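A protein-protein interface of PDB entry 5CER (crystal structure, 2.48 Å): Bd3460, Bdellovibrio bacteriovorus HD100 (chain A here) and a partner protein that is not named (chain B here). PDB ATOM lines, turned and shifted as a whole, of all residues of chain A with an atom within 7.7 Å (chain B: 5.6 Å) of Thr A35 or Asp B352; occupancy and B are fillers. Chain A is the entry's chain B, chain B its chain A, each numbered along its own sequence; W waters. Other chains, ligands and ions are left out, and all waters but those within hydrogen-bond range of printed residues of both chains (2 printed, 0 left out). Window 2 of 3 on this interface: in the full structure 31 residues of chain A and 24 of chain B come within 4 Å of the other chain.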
ATOM      1  N   GLN A  32      19.315 -29.404  -3.650  1.00  0.00           N
ATOM      2  CA  GLN A  32      19.499 -29.068  -5.050  1.00  0.00           C
ATOM      3  C   GLN A  32      18.486 -27.980  -5.408  1.00  0.00           C
ATOM      4  O   GLN A  32      17.364 -28.030  -4.954  1.00  0.00           O
ATOM      5  CB  GLN A  32      19.338 -30.337  -5.939  1.00  0.00           C
ATOM      6  CG  GLN A  32      20.329 -31.462  -5.607  1.00  0.00           C
ATOM      7  CD  GLN A  32      20.173 -32.712  -6.484  1.00  0.00           C
ATOM      8  OE1 GLN A  32      19.414 -33.611  -6.151  1.00  0.00           O
ATOM      9  NE2 GLN A  32      20.838 -32.746  -7.631  1.00  0.00           N
ATOM     10  N   ASP A  33      18.873 -27.050  -6.288  1.00  0.00           N
ATOM     11  CA  ASP A  33      17.986 -25.953  -6.701  1.00  0.00           C
ATOM     12  C   ASP A  33      17.026 -26.402  -7.833  1.00  0.00           C
ATOM     13  O   ASP A  33      16.935 -27.594  -8.138  1.00  0.00           O
ATOM     14  CB  ASP A  33      18.801 -24.705  -7.028  1.00  0.00           C
ATOM     15  CG  ASP A  33      19.503 -24.763  -8.396  1.00  0.00           C
ATOM     16  OD1 ASP A  33      19.390 -25.774  -9.152  1.00  0.00           O
ATOM     17  OD2 ASP A  33      20.187 -23.776  -8.699  1.00  0.00           O
ATOM     18  N   GLU A  34      16.300 -25.477  -8.444  1.00  0.00           N
ATOM     19  CA  GLU A  34      15.296 -25.846  -9.474  1.00  0.00           C
ATOM     20  C   GLU A  34      15.880 -26.503 -10.776  1.00  0.00           C
ATOM     21  O   GLU A  34      15.162 -27.170 -11.483  1.00  0.00           O
ATOM     22  CB  GLU A  34      14.342 -24.655  -9.761  1.00  0.00           C
ATOM     23  CG  GLU A  34      14.938 -23.451 -10.486  1.00  0.00           C
ATOM     24  CD  GLU A  34      15.781 -22.517  -9.606  1.00  0.00           C
ATOM     25  OE1 GLU A  34      15.944 -22.743  -8.371  1.00  0.00           O
ATOM     26  OE2 GLU A  34      16.347 -21.554 -10.181  1.00  0.00           O
ATOM     27  N   THR A  35      17.180 -26.341 -11.052  1.00  0.00           N
ATOM     28  CA  THR A  35      17.880 -27.083 -12.119  1.00  0.00           C
ATOM     29  C   THR A  35      18.795 -28.229 -11.620  1.00  0.00           C
ATOM     30  O   THR A  35      19.580 -28.774 -12.399  1.00  0.00           O
ATOM     31  CB  THR A  35      18.717 -26.143 -12.994  1.00  0.00           C
ATOM     32  OG1 THR A  35      19.884 -25.684 -12.301  1.00  0.00           O
ATOM     33  CG2 THR A  35      17.874 -24.958 -13.435  1.00  0.00           C
ATOM     34  N   GLY A  36      18.654 -28.619 -10.345  1.00  0.00           N
ATOM     35  CA  GLY A  36      19.421 -29.712  -9.775  1.00  0.00           C
ATOM     36  C   GLY A  36      20.805 -29.327  -9.235  1.00  0.00           C
ATOM     37  O   GLY A  36      21.566 -30.214  -8.886  1.00  0.00           O
ATOM     38  N   MET A  37      21.134 -28.032  -9.186  1.00  0.00           N
ATOM     39  CA  MET A  37      22.468 -27.585  -8.791  1.00  0.00           C
ATOM     40  C   MET A  37      22.663 -27.585  -7.267  1.00  0.00           C
ATOM     41  O   MET A  37      21.752 -27.210  -6.513  1.00  0.00           O
ATOM     42  CB  MET A  37      22.754 -26.190  -9.348  1.00  0.00           C
ATOM     43  CG  MET A  37      22.900 -26.125 -10.864  1.00  0.00           C
ATOM     44  SD  MET A  37      24.359 -27.014 -11.422  1.00  0.00           S
ATOM     45  CE  MET A  37      25.679 -25.871 -10.993  1.00  0.00           C
ATOM     46  N   THR A  38      23.855 -28.023  -6.835  1.00  0.00           N
ATOM     47  CA  THR A  38      24.305 -27.973  -5.420  1.00  0.00           C
ATOM     48  C   THR A  38      25.389 -26.905  -5.229  1.00  0.00           C
ATOM     49  O   THR A  38      26.041 -26.490  -6.193  1.00  0.00           O
ATOM     50  CB  THR A  38      24.916 -29.321  -4.956  1.00  0.00           C
ATOM     51  OG1 THR A  38      26.128 -29.601  -5.671  1.00  0.00           O
ATOM     52  CG2 THR A  38      23.951 -30.475  -5.203  1.00  0.00           C
ATOM     53  N   MET A  41      28.661 -28.288  -6.827  1.00  0.00           N
ATOM     54  CA  MET A  41      28.662 -28.114  -8.278  1.00  0.00           C
ATOM     55  C   MET A  41      29.022 -26.672  -8.675  1.00  0.00           C
ATOM     56  O   MET A  41      29.855 -26.450  -9.564  1.00  0.00           O
ATOM     57  CB  MET A  41      27.279 -28.468  -8.869  1.00  0.00           C
ATOM     58  CG  MET A  41      26.917 -29.936  -8.775  1.00  0.00           C
ATOM     59  SD  MET A  41      25.190 -30.176  -9.195  1.00  0.00           S
ATOM     60  CE  MET A  41      24.916 -31.879  -8.675  1.00  0.00           C
ATOM     61  N   ASN A  42      28.399 -25.695  -8.015  1.00  0.00           N
ATOM     62  CA  ASN A  42      28.695 -24.301  -8.298  1.00  0.00           C
ATOM     63  C   ASN A  42      30.160 -23.988  -7.991  1.00  0.00           C
ATOM     64  O   ASN A  42      30.811 -23.303  -8.763  1.00  0.00           O
ATOM     65  CB  ASN A  42      27.776 -23.365  -7.525  1.00  0.00           C
ATOM     66  CG  ASN A  42      26.444 -23.176  -8.196  1.00  0.00           C
ATOM     67  OD1 ASN A  42      26.329 -22.408  -9.127  1.00  0.00           O
ATOM     68  ND2 ASN A  42      25.458 -23.908  -7.765  1.00  0.00           N
ATOM     69  N   LYS A  65      23.572 -35.250  -9.124  1.00  0.00           N
ATOM     70  CA  LYS A  65      23.593 -34.794 -10.511  1.00  0.00           C
ATOM     71  C   LYS A  65      22.613 -33.660 -10.723  1.00  0.00           C
ATOM     72  O   LYS A  65      21.507 -33.692 -10.225  1.00  0.00           O
ATOM     73  CB  LYS A  65      23.236 -35.935 -11.432  1.00  0.00           C
ATOM     74  CG  LYS A  65      24.334 -36.974 -11.497  1.00  0.00           C
ATOM     75  CD  LYS A  65      23.866 -38.269 -12.118  1.00  0.00           C
ATOM     76  CE  LYS A  65      25.090 -39.117 -12.438  1.00  0.00           C
ATOM     77  NZ  LYS A  65      24.737 -40.508 -12.855  1.00  0.00           N
ATOM     78  N   ASN A  66      23.030 -32.651 -11.489  1.00  0.00           N
ATOM     79  CA  ASN A  66      22.099 -31.603 -11.933  1.00  0.00           C
ATOM     80  C   ASN A  66      21.177 -32.130 -13.078  1.00  0.00           C
ATOM     81  O   ASN A  66      21.327 -33.274 -13.514  1.00  0.00           O
ATOM     82  CB  ASN A  66      22.884 -30.354 -12.357  1.00  0.00           C
ATOM     83  CG  ASN A  66      23.439 -30.466 -13.763  1.00  0.00           C
ATOM     84  OD1 ASN A  66      23.943 -31.523 -14.179  1.00  0.00           O
ATOM     85  ND2 ASN A  66      23.331 -29.380 -14.514  1.00  0.00           N
ATOM     86  N   ASN A  67      20.293 -31.296 -13.583  1.00  0.00           N
ATOM     87  CA  ASN A  67      19.417 -31.689 -14.720  1.00  0.00           C
ATOM     88  C   ASN A  67      20.162 -32.200 -15.968  1.00  0.00           C
ATOM     89  O   ASN A  67      19.667 -33.069 -16.664  1.00  0.00           O
ATOM     90  CB  ASN A  67      18.460 -30.557 -15.092  1.00  0.00           C
ATOM     91  CG  ASN A  67      19.153 -29.282 -15.541  1.00  0.00           C
ATOM     92  OD1 ASN A  67      20.390 -29.108 -15.465  1.00  0.00           O
ATOM     93  ND2 ASN A  67      18.337 -28.343 -15.998  1.00  0.00           N
ATOM     94  N   GLY A  68      21.377 -31.688 -16.194  1.00  0.00           N
ATOM     95  CA  GLY A  68      22.248 -32.172 -17.251  1.00  0.00           C
ATOM     96  C   GLY A  68      22.985 -33.489 -17.013  1.00  0.00           C
ATOM     97  O   GLY A  68      23.888 -33.817 -17.798  1.00  0.00           O
ATOM     98  N   GLY A  69      22.694 -34.180 -15.907  1.00  0.00           N
ATOM     99  CA  GLY A  69      23.297 -35.465 -15.601  1.00  0.00           C
ATOM    100  C   GLY A  69      24.711 -35.412 -15.046  1.00  0.00           C
ATOM    101  O   GLY A  69      25.354 -36.460 -14.891  1.00  0.00           O
ATOM    102  N   PHE A  75      31.422 -31.030 -13.565  1.00  0.00           N
ATOM    103  CA  PHE A  75      31.445 -29.555 -13.670  1.00  0.00           C
ATOM    104  C   PHE A  75      32.872 -29.039 -13.629  1.00  0.00           C
ATOM    105  O   PHE A  75      33.249 -28.199 -14.461  1.00  0.00           O
ATOM    106  CB  PHE A  75      30.627 -28.863 -12.587  1.00  0.00           C
ATOM    107  CG  PHE A  75      29.164 -28.779 -12.911  1.00  0.00           C
ATOM    108  CD1 PHE A  75      28.680 -27.751 -13.708  1.00  0.00           C
ATOM    109  CD2 PHE A  75      28.275 -29.743 -12.437  1.00  0.00           C
ATOM    110  CE1 PHE A  75      27.342 -27.677 -14.008  1.00  0.00           C
ATOM    111  CE2 PHE A  75      26.935 -29.668 -12.739  1.00  0.00           C
ATOM    112  CZ  PHE A  75      26.477 -28.615 -13.510  1.00  0.00           C
ATOM    113  N   ASN B 325      25.820 -15.620 -18.117  1.00  0.00           N
ATOM    114  CA  ASN B 325      24.737 -16.589 -18.128  1.00  0.00           C
ATOM    115  C   ASN B 325      24.185 -16.854 -19.539  1.00  0.00           C
ATOM    116  O   ASN B 325      23.857 -17.998 -19.844  1.00  0.00           O
ATOM    117  CB  ASN B 325      23.628 -16.167 -17.196  1.00  0.00           C
ATOM    118  CG  ASN B 325      23.973 -16.378 -15.735  1.00  0.00           C
ATOM    119  OD1 ASN B 325      24.955 -17.025 -15.389  1.00  0.00           O
ATOM    120  ND2 ASN B 325      23.165 -15.808 -14.863  1.00  0.00           N
ATOM    121  N   LYS B 326      24.157 -15.807 -20.378  1.00  0.00           N
ATOM    122  CA  LYS B 326      23.635 -15.901 -21.735  1.00  0.00           C
ATOM    123  C   LYS B 326      24.681 -16.085 -22.850  1.00  0.00           C
ATOM    124  O   LYS B 326      24.310 -16.145 -24.037  1.00  0.00           O
ATOM    125  CB  LYS B 326      22.750 -14.689 -22.065  1.00  0.00           C
ATOM    126  CG  LYS B 326      21.556 -14.551 -21.180  1.00  0.00           C
ATOM    127  CD  LYS B 326      20.705 -15.798 -21.201  1.00  0.00           C
ATOM    128  CE  LYS B 326      19.400 -15.593 -20.494  1.00  0.00           C
ATOM    129  NZ  LYS B 326      18.628 -16.859 -20.393  1.00  0.00           N
ATOM    130  N   ASP B 350      22.163 -20.649 -21.859  1.00  0.00           N
ATOM    131  CA  ASP B 350      21.102 -20.315 -20.853  1.00  0.00           C
ATOM    132  C   ASP B 350      21.302 -21.078 -19.544  1.00  0.00           C
ATOM    133  O   ASP B 350      20.786 -22.185 -19.360  1.00  0.00           O
ATOM    134  CB  ASP B 350      19.678 -20.655 -21.376  1.00  0.00           C
ATOM    135  CG  ASP B 350      19.312 -19.929 -22.688  1.00  0.00           C
ATOM    136  OD1 ASP B 350      18.964 -18.714 -22.607  1.00  0.00           O
ATOM    137  OD2 ASP B 350      19.333 -20.615 -23.740  1.00  0.00           O
ATOM    138  N   MET B 351      22.070 -20.494 -18.641  1.00  0.00           N
ATOM    139  CA  MET B 351      22.319 -21.131 -17.347  1.00  0.00           C
ATOM    140  C   MET B 351      21.058 -21.350 -16.591  1.00  0.00           C
ATOM    141  O   MET B 351      20.959 -22.300 -15.850  1.00  0.00           O
ATOM    142  CB  MET B 351      23.220 -20.293 -16.499  1.00  0.00           C
ATOM    143  CG  MET B 351      24.594 -20.121 -17.094  1.00  0.00           C
ATOM    144  SD  MET B 351      25.525 -21.628 -17.476  1.00  0.00           S
ATOM    145  CE  MET B 351      26.893 -20.665 -18.202  1.00  0.00           C
ATOM    146  N   ASP B 352      20.096 -20.459 -16.754  1.00  0.00           N
ATOM    147  CA  ASP B 352      18.808 -20.645 -16.138  1.00  0.00           C
ATOM    148  C   ASP B 352      18.061 -21.925 -16.609  1.00  0.00           C
ATOM    149  O   ASP B 352      17.174 -22.409 -15.887  1.00  0.00           O
ATOM    150  CB  ASP B 352      17.916 -19.402 -16.318  1.00  0.00           C
ATOM    151  CG  ASP B 352      17.624 -19.106 -17.757  1.00  0.00           C
ATOM    152  OD1 ASP B 352      18.570 -18.839 -18.518  1.00  0.00           O
ATOM    153  OD2 ASP B 352      16.445 -19.164 -18.141  1.00  0.00           O
ATOM    154  N   GLN B 353      18.363 -22.431 -17.794  1.00  0.00           N
ATOM    155  CA  GLN B 353      17.817 -23.705 -18.251  1.00  0.00           C
ATOM    156  C   GLN B 353      18.694 -24.816 -17.724  1.00  0.00           C
ATOM    157  O   GLN B 353      18.193 -25.726 -17.071  1.00  0.00           O
ATOM    158  CB  GLN B 353      17.727 -23.761 -19.779  1.00  0.00           C
ATOM    159  CG  GLN B 353      16.740 -22.775 -20.387  1.00  0.00           C
ATOM    160  CD  GLN B 353      16.861 -22.610 -21.902  1.00  0.00           C
ATOM    161  OE1 GLN B 353      17.287 -23.516 -22.629  1.00  0.00           O
ATOM    162  NE2 GLN B 353      16.438 -21.439 -22.396  1.00  0.00           N
ATOM    163  N   SER B 354      20.019 -24.715 -17.910  1.00  0.00           N
ATOM    164  CA  SER B 354      20.947 -25.636 -17.272  1.00  0.00           C
ATOM    165  C   SER B 354      22.340 -25.052 -17.161  1.00  0.00           C
ATOM    166  O   SER B 354      22.869 -24.504 -18.123  1.00  0.00           O
ATOM    167  CB  SER B 354      21.021 -26.930 -18.056  1.00  0.00           C
ATOM    168  OG  SER B 354      21.841 -27.878 -17.387  1.00  0.00           O
ATOM    169  N   SER B 355      22.957 -25.227 -15.997  1.00  0.00           N
ATOM    170  CA  SER B 355      24.339 -24.849 -15.834  1.00  0.00           C
ATOM    171  C   SER B 355      25.284 -25.727 -16.631  1.00  0.00           C
ATOM    172  O   SER B 355      26.420 -25.322 -16.826  1.00  0.00           O
ATOM    173  CB  SER B 355      24.780 -24.864 -14.371  1.00  0.00           C
ATOM    174  OG  SER B 355      24.103 -23.865 -13.631  1.00  0.00           O
HETATM  175  O   HOH W   1      21.469 -23.487 -13.457  1.00  0.00           O
HETATM  176  O   HOH W   2      21.697 -26.909 -14.100  1.00  0.00           O
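OD2 of Asp B350 lies close to NE2 of Gln B353 (3.3 Å).
The side-chain carboxylate of Asp A33 lies within hydrogen-bond range of the backbone NH of Thr A35, 3.0 Å away.
O of Thr A35 sits at hydrogen-bond distance from N of Asn A67 (2.9 Å).
The side-chain amide nitrogen (ND2) of Asn A66 sits at hydrogen-bond distance from the side-chain amide oxygen (OD1) of Asn A67, 3.1 Å away.
The side-chain amide oxygen (OD1) of Asn A66 sits close to the backbone NH (N) of Gly A68, at 3.3 Å.
The side-chain amide oxygen (OD1) of Asn A66 is in hydrogen-bond range of the backbone NH (N) of Gly A69 (3.4 Å).
Of the 15 printed residues of chain A, 5 touch a printed residue of chain B.
Printed residues of chain A that touch a printed residue of chain B: Thr A35, Met A37, Asn A66, Asn A67 and Phe A75.
Among the printed residues, 7 pairs touch across the chains.
Among the printed residues, no Asp or Glu carboxylate lies within 4 Å of a Lys or Arg side-chain nitrogen of the other chain.
Thr A35 touches just these residues of chain B: Asp B352 (3.6 Å) and Gln B353 (3.7 Å).
Of the printed residues of chain B, Met A37 touches Ser B355.
Printed residues of chain B within 4 Å of Asn A66: Ser B354.
Of the printed residues of chain B, Phe A75 touches Ser B355.
Printed residues of chain A within 4 Å of Gln B353: Thr A35 (3.7 Å) and Asn A67 (2.8 Å).
Printed residues of chain B within 4 Å of Asn A67: Gln B353 and Ser B354.
The nearest residue of chain A that does not touch Asp B352 is Glu A34 (5.8 Å).
O of Gln B353 lies within hydrogen-bond range of ND2 of Asn A67 (2.8 Å).
The side-chain hydroxyl (OG) of Ser B354 is in hydrogen-bond range of the side-chain amide oxygen (OD1) of Asn A67 (2.7 Å).
Among the printed residues, merely in contact across the chains: Asn A66 with Ser B354 (3.6 Å), Thr A35 with Asp B352 (3.6 Å), Met A37 with Ser B355 (3.6 Å), Thr A35 with Gln B353 (3.7 Å) and Phe A75 with Ser B355 (3.8 Å).
Water W1 lies within hydrogen-bond range of the side-chain hydroxyl (OG) of Ser B355, the backbone carbonyl oxygen (O) of Met B351 and the side-chain hydroxyl (OG1) of Thr A35.
Water W2 lies within hydrogen-bond range of the backbone NH (N) of Ser B355 (2.8 Å), the side-chain hydroxyl (OG1) of Thr A35 (2.8 Å), the side-chain amide oxygen (OD1) of Asn A67 (2.9 Å), the side-chain amide nitrogen (ND2) of Asn A66 (3.0 Å), the side-chain hydroxyl (OG) of Ser B354 (3.4 Å) and the side-chain sulfur (SD) of Met A37 (3.8 Å).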
